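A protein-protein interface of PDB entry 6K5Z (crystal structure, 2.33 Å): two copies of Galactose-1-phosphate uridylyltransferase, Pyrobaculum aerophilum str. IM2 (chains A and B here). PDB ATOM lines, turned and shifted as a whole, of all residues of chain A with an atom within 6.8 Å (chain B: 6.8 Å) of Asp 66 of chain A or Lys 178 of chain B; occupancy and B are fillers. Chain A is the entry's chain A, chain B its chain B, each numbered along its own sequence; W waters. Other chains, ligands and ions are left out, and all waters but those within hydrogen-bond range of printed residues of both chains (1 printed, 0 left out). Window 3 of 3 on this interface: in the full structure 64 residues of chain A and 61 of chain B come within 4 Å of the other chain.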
ATOM      1  N   ALA A  64      16.793 -21.341  38.279  1.00  0.00           N
ATOM      2  CA  ALA A  64      17.565 -20.809  37.169  1.00  0.00           C
ATOM      3  C   ALA A  64      16.737 -20.202  36.045  1.00  0.00           C
ATOM      4  O   ALA A  64      15.643 -20.669  35.734  1.00  0.00           O
ATOM      5  CB  ALA A  64      18.492 -21.881  36.615  1.00  0.00           C
ATOM      6  N   GLU A  65      17.283 -19.155  35.440  1.00  0.00           N
ATOM      7  CA  GLU A  65      16.647 -18.507  34.293  1.00  0.00           C
ATOM      8  C   GLU A  65      17.719 -18.278  33.219  1.00  0.00           C
ATOM      9  O   GLU A  65      18.898 -18.132  33.538  1.00  0.00           O
ATOM     10  CB  GLU A  65      15.908 -17.223  34.683  1.00  0.00           C
ATOM     11  CG  GLU A  65      14.956 -16.720  33.605  1.00  0.00           C
ATOM     12  CD  GLU A  65      13.561 -16.419  34.126  1.00  0.00           C
ATOM     13  OE1 GLU A  65      13.101 -17.116  35.052  1.00  0.00           O
ATOM     14  OE2 GLU A  65      12.917 -15.493  33.594  1.00  0.00           O
ATOM     15  N   ASP A  66      17.314 -18.224  31.955  1.00  0.00           N
ATOM     16  CA  ASP A  66      18.273 -18.125  30.850  1.00  0.00           C
ATOM     17  C   ASP A  66      19.214 -16.917  30.742  1.00  0.00           C
ATOM     18  O   ASP A  66      20.395 -17.107  30.457  1.00  0.00           O
ATOM     19  CB  ASP A  66      17.570 -18.365  29.509  1.00  0.00           C
ATOM     20  CG  ASP A  66      18.510 -18.909  28.448  1.00  0.00           C
ATOM     21  OD1 ASP A  66      19.718 -18.602  28.504  1.00  0.00           O
ATOM     22  OD2 ASP A  66      18.041 -19.644  27.555  1.00  0.00           O
ATOM     23  N   LEU A  67      18.751 -15.691  30.968  1.00  0.00           N
ATOM     24  CA  LEU A  67      19.710 -14.567  30.843  1.00  0.00           C
ATOM     25  C   LEU A  67      20.271 -13.958  32.139  1.00  0.00           C
ATOM     26  O   LEU A  67      20.994 -12.939  32.075  1.00  0.00           O
ATOM     27  CB  LEU A  67      19.133 -13.456  29.965  1.00  0.00           C
ATOM     28  CG  LEU A  67      19.301 -13.735  28.469  1.00  0.00           C
ATOM     29  CD1 LEU A  67      18.066 -14.453  27.955  1.00  0.00           C
ATOM     30  CD2 LEU A  67      19.569 -12.473  27.665  1.00  0.00           C
ATOM     31  N   TYR A  68      19.993 -14.594  33.285  1.00  0.00           N
ATOM     32  CA  TYR A  68      20.307 -14.042  34.615  1.00  0.00           C
ATOM     33  C   TYR A  68      21.194 -14.942  35.493  1.00  0.00           C
ATOM     34  O   TYR A  68      21.216 -16.165  35.344  1.00  0.00           O
ATOM     35  CB  TYR A  68      19.007 -13.779  35.374  1.00  0.00           C
ATOM     36  CG  TYR A  68      17.984 -13.060  34.549  1.00  0.00           C
ATOM     37  CD1 TYR A  68      18.149 -11.712  34.236  1.00  0.00           C
ATOM     38  CD2 TYR A  68      16.863 -13.728  34.043  1.00  0.00           C
ATOM     39  CE1 TYR A  68      17.217 -11.043  33.456  1.00  0.00           C
ATOM     40  CE2 TYR A  68      15.926 -13.067  33.261  1.00  0.00           C
ATOM     41  CZ  TYR A  68      16.108 -11.728  32.983  1.00  0.00           C
ATOM     42  OH  TYR A  68      15.171 -11.056  32.257  1.00  0.00           O
ATOM     43  N   GLU A  69      21.893 -14.305  36.430  1.00  0.00           N
ATOM     44  CA  GLU A  69      22.664 -15.008  37.450  1.00  0.00           C
ATOM     45  C   GLU A  69      21.812 -15.185  38.717  1.00  0.00           C
ATOM     46  O   GLU A  69      21.174 -14.238  39.212  1.00  0.00           O
ATOM     47  CB  GLU A  69      23.984 -14.288  37.725  1.00  0.00           C
ATOM     48  CG  GLU A  69      24.884 -14.229  36.492  1.00  0.00           C
ATOM     49  CD  GLU A  69      26.156 -13.422  36.728  1.00  0.00           C
ATOM     50  OE1 GLU A  69      27.245 -14.034  36.905  1.00  0.00           O
ATOM     51  OE2 GLU A  69      26.068 -12.176  36.743  1.00  0.00           O
ATOM     52  N   HIS B 172      18.607  -5.219  26.589  1.00  0.00           N
ATOM     53  CA  HIS B 172      17.221  -4.849  26.867  1.00  0.00           C
ATOM     54  C   HIS B 172      16.327  -5.469  25.791  1.00  0.00           C
ATOM     55  O   HIS B 172      15.442  -6.260  26.118  1.00  0.00           O
ATOM     56  CB  HIS B 172      17.034  -3.322  26.923  1.00  0.00           C
ATOM     57  CG  HIS B 172      17.868  -2.613  27.962  1.00  0.00           C
ATOM     58  ND1 HIS B 172      17.423  -2.380  29.246  1.00  0.00           N
ATOM     59  CD2 HIS B 172      19.085  -2.024  27.881  1.00  0.00           C
ATOM     60  CE1 HIS B 172      18.332  -1.692  29.910  1.00  0.00           C
ATOM     61  NE2 HIS B 172      19.353  -1.466  29.108  1.00  0.00           N
ATOM     62  N   CYS B 173      16.584  -5.165  24.516  1.00  0.00           N
ATOM     63  CA  CYS B 173      15.835  -5.839  23.425  1.00  0.00           C
ATOM     64  C   CYS B 173      15.793  -7.344  23.656  1.00  0.00           C
ATOM     65  O   CYS B 173      14.724  -7.953  23.669  1.00  0.00           O
ATOM     66  CB  CYS B 173      16.483  -5.609  22.075  1.00  0.00           C
ATOM     67  SG  CYS B 173      16.407  -3.925  21.500  1.00  0.00           S
ATOM     68  N   ARG B 174      16.946  -7.932  23.946  1.00  0.00           N
ATOM     69  CA  ARG B 174      17.001  -9.369  24.152  1.00  0.00           C
ATOM     70  C   ARG B 174      16.094  -9.758  25.311  1.00  0.00           C
ATOM     71  O   ARG B 174      15.363 -10.743  25.227  1.00  0.00           O
ATOM     72  CB  ARG B 174      18.442  -9.799  24.436  1.00  0.00           C
ATOM     73  CG  ARG B 174      18.627 -11.284  24.705  1.00  0.00           C
ATOM     74  CD  ARG B 174      18.461 -12.114  23.442  1.00  0.00           C
ATOM     75  NE  ARG B 174      18.785 -13.520  23.668  1.00  0.00           N
ATOM     76  CZ  ARG B 174      17.929 -14.414  24.153  1.00  0.00           C
ATOM     77  NH1 ARG B 174      16.694 -14.049  24.466  1.00  0.00           N
ATOM     78  NH2 ARG B 174      18.308 -15.673  24.327  1.00  0.00           N
ATOM     79  N   ILE B 175      16.135  -8.988  26.392  1.00  0.00           N
ATOM     80  CA  ILE B 175      15.279  -9.266  27.540  1.00  0.00           C
ATOM     81  C   ILE B 175      13.791  -9.104  27.224  1.00  0.00           C
ATOM     82  O   ILE B 175      12.969  -9.932  27.612  1.00  0.00           O
ATOM     83  CB  ILE B 175      15.612  -8.345  28.729  1.00  0.00           C
ATOM     84  CG1 ILE B 175      17.036  -8.599  29.224  1.00  0.00           C
ATOM     85  CG2 ILE B 175      14.615  -8.548  29.856  1.00  0.00           C
ATOM     86  CD1 ILE B 175      17.421  -7.751  30.415  1.00  0.00           C
ATOM     87  N   VAL B 176      13.452  -8.032  26.516  1.00  0.00           N
ATOM     88  CA  VAL B 176      12.059  -7.757  26.177  1.00  0.00           C
ATOM     89  C   VAL B 176      11.413  -8.790  25.260  1.00  0.00           C
ATOM     90  O   VAL B 176      10.290  -9.226  25.504  1.00  0.00           O
ATOM     91  CB  VAL B 176      11.911  -6.367  25.528  1.00  0.00           C
ATOM     92  CG1 VAL B 176      10.518  -6.199  24.943  1.00  0.00           C
ATOM     93  CG2 VAL B 176      12.214  -5.272  26.538  1.00  0.00           C
ATOM     94  N   GLU B 177      12.130  -9.187  24.215  1.00  0.00           N
ATOM     95  CA  GLU B 177      11.610 -10.163  23.261  1.00  0.00           C
ATOM     96  C   GLU B 177      11.393 -11.539  23.874  1.00  0.00           C
ATOM     97  O   GLU B 177      10.407 -12.213  23.586  1.00  0.00           O
ATOM     98  CB  GLU B 177      12.512 -10.259  22.029  1.00  0.00           C
ATOM     99  CG  GLU B 177      11.923 -11.107  20.913  1.00  0.00           C
ATOM    100  CD  GLU B 177      10.490 -10.731  20.586  1.00  0.00           C
ATOM    101  OE1 GLU B 177      10.110  -9.564  20.817  1.00  0.00           O
ATOM    102  OE2 GLU B 177       9.741 -11.603  20.097  1.00  0.00           O
ATOM    103  N   LYS B 178      12.327 -11.949  24.721  1.00  0.00           N
ATOM    104  CA  LYS B 178      12.264 -13.255  25.359  1.00  0.00           C
ATOM    105  C   LYS B 178      11.145 -13.360  26.388  1.00  0.00           C
ATOM    106  O   LYS B 178      10.474 -14.383  26.487  1.00  0.00           O
ATOM    107  CB  LYS B 178      13.607 -13.597  26.009  1.00  0.00           C
ATOM    108  CG  LYS B 178      13.818 -15.082  26.249  1.00  0.00           C
ATOM    109  CD  LYS B 178      15.215 -15.366  26.773  1.00  0.00           C
ATOM    110  CE  LYS B 178      15.558 -16.841  26.648  1.00  0.00           C
ATOM    111  NZ  LYS B 178      14.557 -17.709  27.327  1.00  0.00           N
ATOM    112  N   GLU B 179      10.952 -12.294  27.154  1.00  0.00           N
ATOM    113  CA  GLU B 179       9.942 -12.286  28.206  1.00  0.00           C
ATOM    114  C   GLU B 179       8.500 -12.377  27.724  1.00  0.00           C
ATOM    115  O   GLU B 179       8.062 -11.586  26.891  1.00  0.00           O
ATOM    116  CB  GLU B 179      10.101 -11.013  29.041  1.00  0.00           C
ATOM    117  CG  GLU B 179       9.136 -10.905  30.206  1.00  0.00           C
ATOM    118  CD  GLU B 179       9.545 -11.777  31.371  1.00  0.00           C
ATOM    119  OE1 GLU B 179       8.801 -12.725  31.696  1.00  0.00           O
ATOM    120  OE2 GLU B 179      10.618 -11.520  31.953  1.00  0.00           O
ATOM    121  N   GLU B 180       7.768 -13.356  28.252  1.00  0.00           N
ATOM    122  CA  GLU B 180       6.355 -13.500  27.927  1.00  0.00           C
ATOM    123  C   GLU B 180       5.529 -14.083  29.076  1.00  0.00           C
ATOM    124  O   GLU B 180       4.363 -13.738  29.247  1.00  0.00           O
ATOM    125  CB  GLU B 180       6.169 -14.319  26.650  1.00  0.00           C
ATOM    126  CG  GLU B 180       4.865 -14.022  25.931  1.00  0.00           C
ATOM    127  CD  GLU B 180       5.009 -14.077  24.425  1.00  0.00           C
ATOM    128  OE1 GLU B 180       5.578 -15.065  23.919  1.00  0.00           O
ATOM    129  OE2 GLU B 180       4.554 -13.128  23.752  1.00  0.00           O
ATOM    130  N   LYS B 181       6.143 -14.965  29.862  1.00  0.00           N
ATOM    131  CA  LYS B 181       5.464 -15.586  31.000  1.00  0.00           C
ATOM    132  C   LYS B 181       5.108 -14.570  32.076  1.00  0.00           C
ATOM    133  O   LYS B 181       4.045 -14.641  32.691  1.00  0.00           O
ATOM    134  CB  LYS B 181       6.299 -16.717  31.601  1.00  0.00           C
ATOM    135  CG  LYS B 181       5.754 -17.228  32.925  1.00  0.00           C
ATOM    136  CD  LYS B 181       6.455 -18.500  33.374  1.00  0.00           C
ATOM    137  CE  LYS B 181       5.962 -19.706  32.592  1.00  0.00           C
ATOM    138  NZ  LYS B 181       4.523 -19.980  32.855  1.00  0.00           N
ATOM    139  N   LYS B 191       5.755  -3.260  25.634  1.00  0.00           N
ATOM    140  CA  LYS B 191       5.649  -4.415  26.485  1.00  0.00           C
ATOM    141  C   LYS B 191       5.852  -4.009  27.984  1.00  0.00           C
ATOM    142  O   LYS B 191       6.764  -3.241  28.324  1.00  0.00           O
ATOM    143  CB  LYS B 191       6.645  -5.468  26.005  1.00  0.00           C
ATOM    144  CG  LYS B 191       6.165  -6.871  26.280  1.00  0.00           C
ATOM    145  CD  LYS B 191       7.140  -7.947  25.811  1.00  0.00           C
ATOM    146  CE  LYS B 191       6.786  -8.530  24.449  1.00  0.00           C
ATOM    147  NZ  LYS B 191       7.527  -9.794  24.217  1.00  0.00           N
HETATM  148  O   HOH W   1      13.339 -11.956  30.139  1.00  0.00           O
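Water W1 lies within hydrogen-bond range of the side-chain hydroxyl of Tyr 68 of chain A (2.9 Å), the backbone carbonyl oxygen of Ile 175 of chain B (3.3 Å) and the side-chain carboxylate of Glu 179 of chain B (3.3 Å).
Among the printed residues, pairs that only touch across the chains: Leu 67 of chain A with Arg 174 of chain B (3.3 Å), Leu 67 of chain A with Lys 178 of chain B (3.2 Å) and Tyr 68 of chain A with Ile 175 of chain B (3.5 Å).
The side-chain carboxylate of Asp 66 of chain A lies within salt-bridge range of the side-chain amino group of Lys 178 of chain B (3.99 Å).
Of chain B, only Lys 178 (3.8 Å) comes within 4 Å of Asp 66 of chain A. Printed residues of chain B within 4 Å of Leu 67 of chain A: Arg 174 and Lys 178. Printed residues of chain A within 4 Å of Arg 174 of chain B: Leu 67. Lys 178 of chain B touches just these residues of chain A: Asp 66 and Leu 67. The nearest residue of chain B that does not touch Asp 66 of chain A is Arg 174 of chain B (5.1 Å). The nearest printed residue of chain A that does not touch Arg 174 of chain B is Asp 66 of chain A (5.1 Å).
Of the 11 printed residues of chain B, 3 touch a printed residue of chain A. Hydrophobic or aromatic side chains of chain A that line the printed part of chain B: Leu 67 and Tyr 68.
No position is printed for both chains.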
